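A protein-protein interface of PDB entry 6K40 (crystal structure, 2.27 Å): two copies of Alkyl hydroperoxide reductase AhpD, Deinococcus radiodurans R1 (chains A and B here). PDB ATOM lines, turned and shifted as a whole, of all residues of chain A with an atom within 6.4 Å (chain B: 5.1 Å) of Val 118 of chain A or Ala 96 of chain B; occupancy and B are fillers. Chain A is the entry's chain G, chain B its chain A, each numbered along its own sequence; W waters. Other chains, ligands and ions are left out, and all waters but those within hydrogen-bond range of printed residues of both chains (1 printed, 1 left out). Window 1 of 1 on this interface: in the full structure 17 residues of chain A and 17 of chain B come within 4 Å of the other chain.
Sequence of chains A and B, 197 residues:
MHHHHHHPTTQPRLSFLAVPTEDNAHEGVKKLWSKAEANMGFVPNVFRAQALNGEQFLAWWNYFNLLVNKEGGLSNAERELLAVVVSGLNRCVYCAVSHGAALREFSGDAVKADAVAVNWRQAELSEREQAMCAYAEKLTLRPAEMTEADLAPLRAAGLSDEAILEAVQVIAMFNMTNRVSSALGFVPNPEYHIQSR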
ATOM      1  N   VAL A  84     -20.376 -30.336 -12.377  1.00  0.00           N
ATOM      2  CA  VAL A  84     -19.876 -29.516 -11.282  1.00  0.00           C
ATOM      3  C   VAL A  84     -18.403 -29.185 -11.491  1.00  0.00           C
ATOM      4  O   VAL A  84     -17.986 -28.033 -11.313  1.00  0.00           O
ATOM      5  CB  VAL A  84     -20.131 -30.229  -9.942  1.00  0.00           C
ATOM      6  CG1 VAL A  84     -19.243 -29.678  -8.861  1.00  0.00           C
ATOM      7  CG2 VAL A  84     -21.593 -30.089  -9.547  1.00  0.00           C
ATOM      8  N   GLY A  88     -17.177 -25.367 -12.208  1.00  0.00           N
ATOM      9  CA  GLY A  88     -16.217 -24.750 -11.311  1.00  0.00           C
ATOM     10  C   GLY A  88     -14.997 -24.243 -12.050  1.00  0.00           C
ATOM     11  O   GLY A  88     -14.492 -23.155 -11.757  1.00  0.00           O
ATOM     12  N   LEU A  89     -14.515 -25.012 -13.030  1.00  0.00           N
ATOM     13  CA  LEU A  89     -13.341 -24.582 -13.784  1.00  0.00           C
ATOM     14  C   LEU A  89     -13.635 -23.336 -14.612  1.00  0.00           C
ATOM     15  O   LEU A  89     -12.836 -22.393 -14.626  1.00  0.00           O
ATOM     16  CB  LEU A  89     -12.842 -25.716 -14.674  1.00  0.00           C
ATOM     17  CG  LEU A  89     -12.175 -26.855 -13.900  1.00  0.00           C
ATOM     18  CD1 LEU A  89     -11.921 -28.041 -14.802  1.00  0.00           C
ATOM     19  CD2 LEU A  89     -10.878 -26.372 -13.268  1.00  0.00           C
ATOM     20  N   ALA A 113     -19.860 -33.076  -2.772  1.00  0.00           N
ATOM     21  CA  ALA A 113     -20.249 -32.111  -3.794  1.00  0.00           C
ATOM     22  C   ALA A 113     -19.516 -30.788  -3.605  1.00  0.00           C
ATOM     23  O   ALA A 113     -18.979 -30.219  -4.565  1.00  0.00           O
ATOM     24  CB  ALA A 113     -21.763 -31.900  -3.765  1.00  0.00           C
ATOM     25  N   ASP A 114     -19.475 -30.289  -2.365  1.00  0.00           N
ATOM     26  CA  ASP A 114     -18.772 -29.040  -2.088  1.00  0.00           C
ATOM     27  C   ASP A 114     -17.294 -29.154  -2.427  1.00  0.00           C
ATOM     28  O   ASP A 114     -16.701 -28.219  -2.979  1.00  0.00           O
ATOM     29  CB  ASP A 114     -18.941 -28.646  -0.619  1.00  0.00           C
ATOM     30  CG  ASP A 114     -20.369 -28.273  -0.266  1.00  0.00           C
ATOM     31  OD1 ASP A 114     -21.200 -28.117  -1.187  1.00  0.00           O
ATOM     32  OD2 ASP A 114     -20.659 -28.127   0.939  1.00  0.00           O
ATOM     33  N   ALA A 115     -16.680 -30.297  -2.110  1.00  0.00           N
ATOM     34  CA  ALA A 115     -15.258 -30.480  -2.384  1.00  0.00           C
ATOM     35  C   ALA A 115     -14.985 -30.540  -3.882  1.00  0.00           C
ATOM     36  O   ALA A 115     -14.037 -29.921  -4.376  1.00  0.00           O
ATOM     37  CB  ALA A 115     -14.750 -31.744  -1.690  1.00  0.00           C
ATOM     38  N   VAL A 116     -15.802 -31.293  -4.621  1.00  0.00           N
ATOM     39  CA  VAL A 116     -15.600 -31.424  -6.059  1.00  0.00           C
ATOM     40  C   VAL A 116     -15.863 -30.099  -6.773  1.00  0.00           C
ATOM     41  O   VAL A 116     -15.236 -29.805  -7.801  1.00  0.00           O
ATOM     42  CB  VAL A 116     -16.491 -32.560  -6.595  1.00  0.00           C
ATOM     43  CG1 VAL A 116     -16.852 -32.336  -8.043  1.00  0.00           C
ATOM     44  CG2 VAL A 116     -15.798 -33.894  -6.420  1.00  0.00           C
ATOM     45  N   ALA A 117     -16.755 -29.262  -6.232  1.00  0.00           N
ATOM     46  CA  ALA A 117     -17.008 -27.961  -6.846  1.00  0.00           C
ATOM     47  C   ALA A 117     -15.763 -27.084  -6.861  1.00  0.00           C
ATOM     48  O   ALA A 117     -15.614 -26.232  -7.745  1.00  0.00           O
ATOM     49  CB  ALA A 117     -18.149 -27.251  -6.117  1.00  0.00           C
ATOM     50  N   VAL A 118     -14.858 -27.281  -5.905  1.00  0.00           N
ATOM     51  CA  VAL A 118     -13.659 -26.458  -5.786  1.00  0.00           C
ATOM     52  C   VAL A 118     -12.463 -27.181  -6.396  1.00  0.00           C
ATOM     53  O   VAL A 118     -11.787 -26.645  -7.283  1.00  0.00           O
ATOM     54  CB  VAL A 118     -13.397 -26.080  -4.317  1.00  0.00           C
ATOM     55  CG1 VAL A 118     -12.071 -25.359  -4.182  1.00  0.00           C
ATOM     56  CG2 VAL A 118     -14.530 -25.214  -3.788  1.00  0.00           C
ATOM     57  N   ASN A 119     -12.176 -28.388  -5.906  1.00  0.00           N
ATOM     58  CA  ASN A 119     -11.023 -29.150  -6.385  1.00  0.00           C
ATOM     59  C   ASN A 119     -11.294 -30.628  -6.139  1.00  0.00           C
ATOM     60  O   ASN A 119     -11.292 -31.072  -4.985  1.00  0.00           O
ATOM     61  CB  ASN A 119      -9.744 -28.700  -5.688  1.00  0.00           C
ATOM     62  CG  ASN A 119      -8.492 -29.032  -6.485  1.00  0.00           C
ATOM     63  OD1 ASN A 119      -8.465 -29.994  -7.253  1.00  0.00           O
ATOM     64  ND2 ASN A 119      -7.446 -28.237  -6.299  1.00  0.00           N
ATOM     65  N   TRP A 120     -11.514 -31.384  -7.217  1.00  0.00           N
ATOM     66  CA  TRP A 120     -11.762 -32.815  -7.082  1.00  0.00           C
ATOM     67  C   TRP A 120     -10.568 -33.552  -6.491  1.00  0.00           C
ATOM     68  O   TRP A 120     -10.746 -34.635  -5.919  1.00  0.00           O
ATOM     69  CB  TRP A 120     -12.125 -33.415  -8.443  1.00  0.00           C
ATOM     70  CG  TRP A 120     -11.065 -33.207  -9.485  1.00  0.00           C
ATOM     71  CD1 TRP A 120     -10.970 -32.164 -10.358  1.00  0.00           C
ATOM     72  CD2 TRP A 120      -9.947 -34.062  -9.755  1.00  0.00           C
ATOM     73  NE1 TRP A 120      -9.862 -32.316 -11.157  1.00  0.00           N
ATOM     74  CE2 TRP A 120      -9.217 -33.473 -10.806  1.00  0.00           C
ATOM     75  CE3 TRP A 120      -9.496 -35.269  -9.213  1.00  0.00           C
ATOM     76  CZ2 TRP A 120      -8.061 -34.050 -11.328  1.00  0.00           C
ATOM     77  CZ3 TRP A 120      -8.345 -35.842  -9.732  1.00  0.00           C
ATOM     78  CH2 TRP A 120      -7.641 -35.233 -10.778  1.00  0.00           C
ATOM     79  N   GLN A 122      -9.017 -32.769  -3.887  1.00  0.00           N
ATOM     80  CA  GLN A 122      -9.153 -32.710  -2.439  1.00  0.00           C
ATOM     81  C   GLN A 122     -10.493 -33.263  -1.966  1.00  0.00           C
ATOM     82  O   GLN A 122     -10.979 -32.889  -0.894  1.00  0.00           O
ATOM     83  CB  GLN A 122      -8.952 -31.275  -1.950  1.00  0.00           C
ATOM     84  CG  GLN A 122      -7.597 -30.686  -2.327  1.00  0.00           C
ATOM     85  CD  GLN A 122      -7.557 -29.173  -2.219  1.00  0.00           C
ATOM     86  OE1 GLN A 122      -8.319 -28.570  -1.462  1.00  0.00           O
ATOM     87  NE2 GLN A 122      -6.663 -28.548  -2.978  1.00  0.00           N
ATOM     88  N   VAL B  84     -12.834 -15.677   0.391  1.00  0.00           N
ATOM     89  CA  VAL B  84     -13.617 -16.569  -0.454  1.00  0.00           C
ATOM     90  C   VAL B  84     -13.193 -16.434  -1.910  1.00  0.00           C
ATOM     91  O   VAL B  84     -13.021 -17.438  -2.614  1.00  0.00           O
ATOM     92  CB  VAL B  84     -15.118 -16.286  -0.258  1.00  0.00           C
ATOM     93  CG1 VAL B  84     -15.929 -16.871  -1.393  1.00  0.00           C
ATOM     94  CG2 VAL B  84     -15.590 -16.837   1.082  1.00  0.00           C
ATOM     95  N   SER B  87      -9.678 -18.062  -2.284  1.00  0.00           N
ATOM     96  CA  SER B  87      -9.712 -19.509  -2.134  1.00  0.00           C
ATOM     97  C   SER B  87     -10.396 -20.181  -3.315  1.00  0.00           C
ATOM     98  O   SER B  87      -9.996 -21.280  -3.715  1.00  0.00           O
ATOM     99  CB  SER B  87     -10.417 -19.857  -0.823  1.00  0.00           C
ATOM    100  OG  SER B  87      -9.730 -19.269   0.267  1.00  0.00           O
ATOM    101  N   ARG B  91      -8.476 -22.628  -5.716  1.00  0.00           N
ATOM    102  CA  ARG B  91      -9.131 -23.930  -5.604  1.00  0.00           C
ATOM    103  C   ARG B  91      -8.655 -24.689  -4.368  1.00  0.00           C
ATOM    104  O   ARG B  91      -8.216 -25.838  -4.444  1.00  0.00           O
ATOM    105  CB  ARG B  91      -8.931 -24.760  -6.877  1.00  0.00           C
ATOM    106  CG  ARG B  91      -9.590 -24.144  -8.095  1.00  0.00           C
ATOM    107  CD  ARG B  91      -9.232 -24.882  -9.363  1.00  0.00           C
ATOM    108  NE  ARG B  91      -9.810 -26.220  -9.399  1.00  0.00           N
ATOM    109  CZ  ARG B  91      -9.408 -27.178 -10.227  1.00  0.00           C
ATOM    110  NH1 ARG B  91      -8.424 -26.942 -11.087  1.00  0.00           N
ATOM    111  NH2 ARG B  91      -9.987 -28.372 -10.196  1.00  0.00           N
ATOM    112  N   CYS B  92      -8.755 -24.035  -3.216  1.00  0.00           N
ATOM    113  CA  CYS B  92      -8.429 -24.658  -1.941  1.00  0.00           C
ATOM    114  C   CYS B  92      -9.723 -25.015  -1.220  1.00  0.00           C
ATOM    115  O   CYS B  92     -10.487 -24.123  -0.835  1.00  0.00           O
ATOM    116  CB  CYS B  92      -7.572 -23.720  -1.090  1.00  0.00           C
ATOM    117  SG  CYS B  92      -7.271 -24.330   0.572  1.00  0.00           S
ATOM    118  N   VAL B  93      -9.961 -26.317  -1.037  1.00  0.00           N
ATOM    119  CA  VAL B  93     -11.234 -26.770  -0.482  1.00  0.00           C
ATOM    120  C   VAL B  93     -11.367 -26.358   0.978  1.00  0.00           C
ATOM    121  O   VAL B  93     -12.434 -25.913   1.414  1.00  0.00           O
ATOM    122  CB  VAL B  93     -11.384 -28.290  -0.657  1.00  0.00           C
ATOM    123  CG1 VAL B  93     -12.563 -28.808   0.149  1.00  0.00           C
ATOM    124  CG2 VAL B  93     -11.543 -28.639  -2.128  1.00  0.00           C
ATOM    125  N   TYR B  94     -10.295 -26.510   1.761  1.00  0.00           N
ATOM    126  CA  TYR B  94     -10.357 -26.148   3.174  1.00  0.00           C
ATOM    127  C   TYR B  94     -10.779 -24.696   3.337  1.00  0.00           C
ATOM    128  O   TYR B  94     -11.754 -24.390   4.043  1.00  0.00           O
ATOM    129  CB  TYR B  94      -9.007 -26.388   3.860  1.00  0.00           C
ATOM    130  CG  TYR B  94      -9.080 -26.279   5.374  1.00  0.00           C
ATOM    131  CD1 TYR B  94      -9.161 -25.040   6.009  1.00  0.00           C
ATOM    132  CD2 TYR B  94      -9.085 -27.418   6.166  1.00  0.00           C
ATOM    133  CE1 TYR B  94      -9.242 -24.946   7.391  1.00  0.00           C
ATOM    134  CE2 TYR B  94      -9.164 -27.333   7.543  1.00  0.00           C
ATOM    135  CZ  TYR B  94      -9.241 -26.098   8.148  1.00  0.00           C
ATOM    136  OH  TYR B  94      -9.321 -26.016   9.515  1.00  0.00           O
ATOM    137  N   CYS B  95     -10.052 -23.784   2.684  1.00  0.00           N
ATOM    138  CA  CYS B  95     -10.341 -22.371   2.866  1.00  0.00           C
ATOM    139  C   CYS B  95     -11.668 -21.999   2.221  1.00  0.00           C
ATOM    140  O   CYS B  95     -12.444 -21.238   2.803  1.00  0.00           O
ATOM    141  CB  CYS B  95      -9.195 -21.526   2.295  1.00  0.00           C
ATOM    142  SG  CYS B  95      -7.590 -21.748   3.106  1.00  0.00           S
ATOM    143  N   ALA B  96     -11.990 -22.595   1.072  1.00  0.00           N
ATOM    144  CA  ALA B  96     -13.289 -22.346   0.453  1.00  0.00           C
ATOM    145  C   ALA B  96     -14.422 -22.679   1.411  1.00  0.00           C
ATOM    146  O   ALA B  96     -15.269 -21.832   1.697  1.00  0.00           O
ATOM    147  CB  ALA B  96     -13.438 -23.141  -0.849  1.00  0.00           C
ATOM    148  N   VAL B  97     -14.416 -23.889   1.971  1.00  0.00           N
ATOM    149  CA  VAL B  97     -15.511 -24.312   2.840  1.00  0.00           C
ATOM    150  C   VAL B  97     -15.566 -23.456   4.103  1.00  0.00           C
ATOM    151  O   VAL B  97     -16.610 -22.873   4.435  1.00  0.00           O
ATOM    152  CB  VAL B  97     -15.376 -25.807   3.176  1.00  0.00           C
ATOM    153  CG1 VAL B  97     -16.390 -26.207   4.232  1.00  0.00           C
ATOM    154  CG2 VAL B  97     -15.549 -26.649   1.916  1.00  0.00           C
ATOM    155  N   SER B  98     -14.444 -23.359   4.830  1.00  0.00           N
ATOM    156  CA  SER B  98     -14.486 -22.691   6.131  1.00  0.00           C
ATOM    157  C   SER B  98     -14.784 -21.199   5.986  1.00  0.00           C
ATOM    158  O   SER B  98     -15.651 -20.654   6.684  1.00  0.00           O
ATOM    159  CB  SER B  98     -13.180 -22.924   6.895  1.00  0.00           C
ATOM    160  OG  SER B  98     -12.049 -22.582   6.121  1.00  0.00           O
ATOM    161  N   HIS B  99     -14.091 -20.514   5.076  1.00  0.00           N
ATOM    162  CA  HIS B  99     -14.323 -19.089   4.935  1.00  0.00           C
ATOM    163  C   HIS B  99     -15.585 -18.771   4.143  1.00  0.00           C
ATOM    164  O   HIS B  99     -16.110 -17.665   4.279  1.00  0.00           O
ATOM    165  CB  HIS B  99     -13.086 -18.439   4.319  1.00  0.00           C
ATOM    166  CG  HIS B  99     -11.883 -18.527   5.206  1.00  0.00           C
ATOM    167  ND1 HIS B  99     -11.688 -17.685   6.279  1.00  0.00           N
ATOM    168  CD2 HIS B  99     -10.838 -19.390   5.211  1.00  0.00           C
ATOM    169  CE1 HIS B  99     -10.563 -18.008   6.892  1.00  0.00           C
ATOM    170  NE2 HIS B  99     -10.029 -19.041   6.265  1.00  0.00           N
ATOM    171  N   GLY B 100     -16.141 -19.726   3.395  1.00  0.00           N
ATOM    172  CA  GLY B 100     -17.482 -19.540   2.878  1.00  0.00           C
ATOM    173  C   GLY B 100     -18.515 -19.588   3.982  1.00  0.00           C
ATOM    174  O   GLY B 100     -19.476 -18.816   3.982  1.00  0.00           O
ATOM    175  N   ALA B 101     -18.331 -20.497   4.943  1.00  0.00           N
ATOM    176  CA  ALA B 101     -19.178 -20.479   6.132  1.00  0.00           C
ATOM    177  C   ALA B 101     -19.066 -19.138   6.848  1.00  0.00           C
ATOM    178  O   ALA B 101     -20.077 -18.537   7.239  1.00  0.00           O
ATOM    179  CB  ALA B 101     -18.796 -21.626   7.067  1.00  0.00           C
HETATM  180  O   HOH W   1      -7.486 -28.030   1.214  1.00  0.00           O
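NE of Arg 91 of chain B is in hydrogen-bond range of O of Val 118 of chain A (2.9 Å).
The backbone carbonyl oxygen (O) of Arg 91 of chain B is in hydrogen-bond range of the side-chain amide nitrogen (ND2) of Asn 119 of chain A (3.1 Å).
The backbone carbonyl oxygen (O) of Arg 91 of chain B lies within hydrogen-bond range of the side-chain amide nitrogen (NE2) of Gln 122 of chain A, at 3.5 Å.
The backbone NH (N) of Val 93 of chain B is in hydrogen-bond range of the side-chain amide oxygen (OE1) of Gln 122 of chain A, 2.8 Å away.
N of Cys 92 of chain B sits at hydrogen-bond distance from O of Ser 87 of chain B (3.1 Å).
The side-chain sulfur of Cys 92 of chain B lies within hydrogen-bond range of the backbone NH of Cys 95 of chain B (3.5 Å).
NE2 of Gln 122 of chain A lies close to ND2 of Asn 119 of chain A.
Position printed for both chains: 84.
Printed residues of chain A that touch a printed residue of chain B: Leu 89, Ala 115, Val 118, Asn 119, Trp 120 and Gln 122.
Hydrophobic or aromatic side chains of chain B within 4 Å of the printed part of chain A: Val 93 and Ala 96.
Among the printed residues, 12 pairs touch across the chains.
Among the printed residues, no Asp or Glu carboxylate lies within 4 Å of a Lys or Arg side-chain nitrogen of the other chain.
Water W1 lies within hydrogen-bond range of OE1 of Gln 122 of chain A (2.9 Å), N of Tyr 94 of chain B (3.2 Å) and SG of Cys 92 of chain B (3.8 Å).
Arg 91 of chain B touches Leu 89 of chain A (NH1 to CD2, 3.3 Å).
CG2 of Val 93 of chain B touches O of Ala 115 of chain A (3.6 Å).
CG1 of Val 118 of chain A touches N of Cys 92 of chain B (3.7 Å).
Val 118 of chain A touches Val 93 of chain B (CB to CG2, 3.8 Å).
CB of Ala 96 of chain B touches CG2 of Val 118 of chain A, 3.8 Å away.
CG2 of Val 93 of chain B touches O of Asn 119 of chain A, at 3.8 Å.
Arg 91 of chain B touches Trp 120 of chain A.
Cys 92 of chain B touches Gln 122 of chain A (C to OE1, 3.8 Å).
Of chain B, only Arg 91 (2.9 Å), Cys 92 (3.7 Å), Val 93 (3.8 Å) and Ala 96 (3.8 Å) come within 4 Å of Val 118 of chain A.
Of chain A, only Val 118 comes within 4 Å of Ala 96 of chain B.
Of the printed residues of chain B, Ala 115 of chain A touches Val 93.
Of the printed residues of chain B, Leu 89 of chain A touches Arg 91.
Printed residues of chain B within 4 Å of Gln 122 of chain A: Arg 91 (3.5 Å), Cys 92 (3.8 Å) and Val 93 (2.8 Å).
The nearest residue of chain B that does not touch Val 118 of chain A is Ser 87 of chain B (4.6 Å).
The nearest printed residue of chain A that does not touch Ala 96 of chain B is Asp 114 of chain A (6.4 Å).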
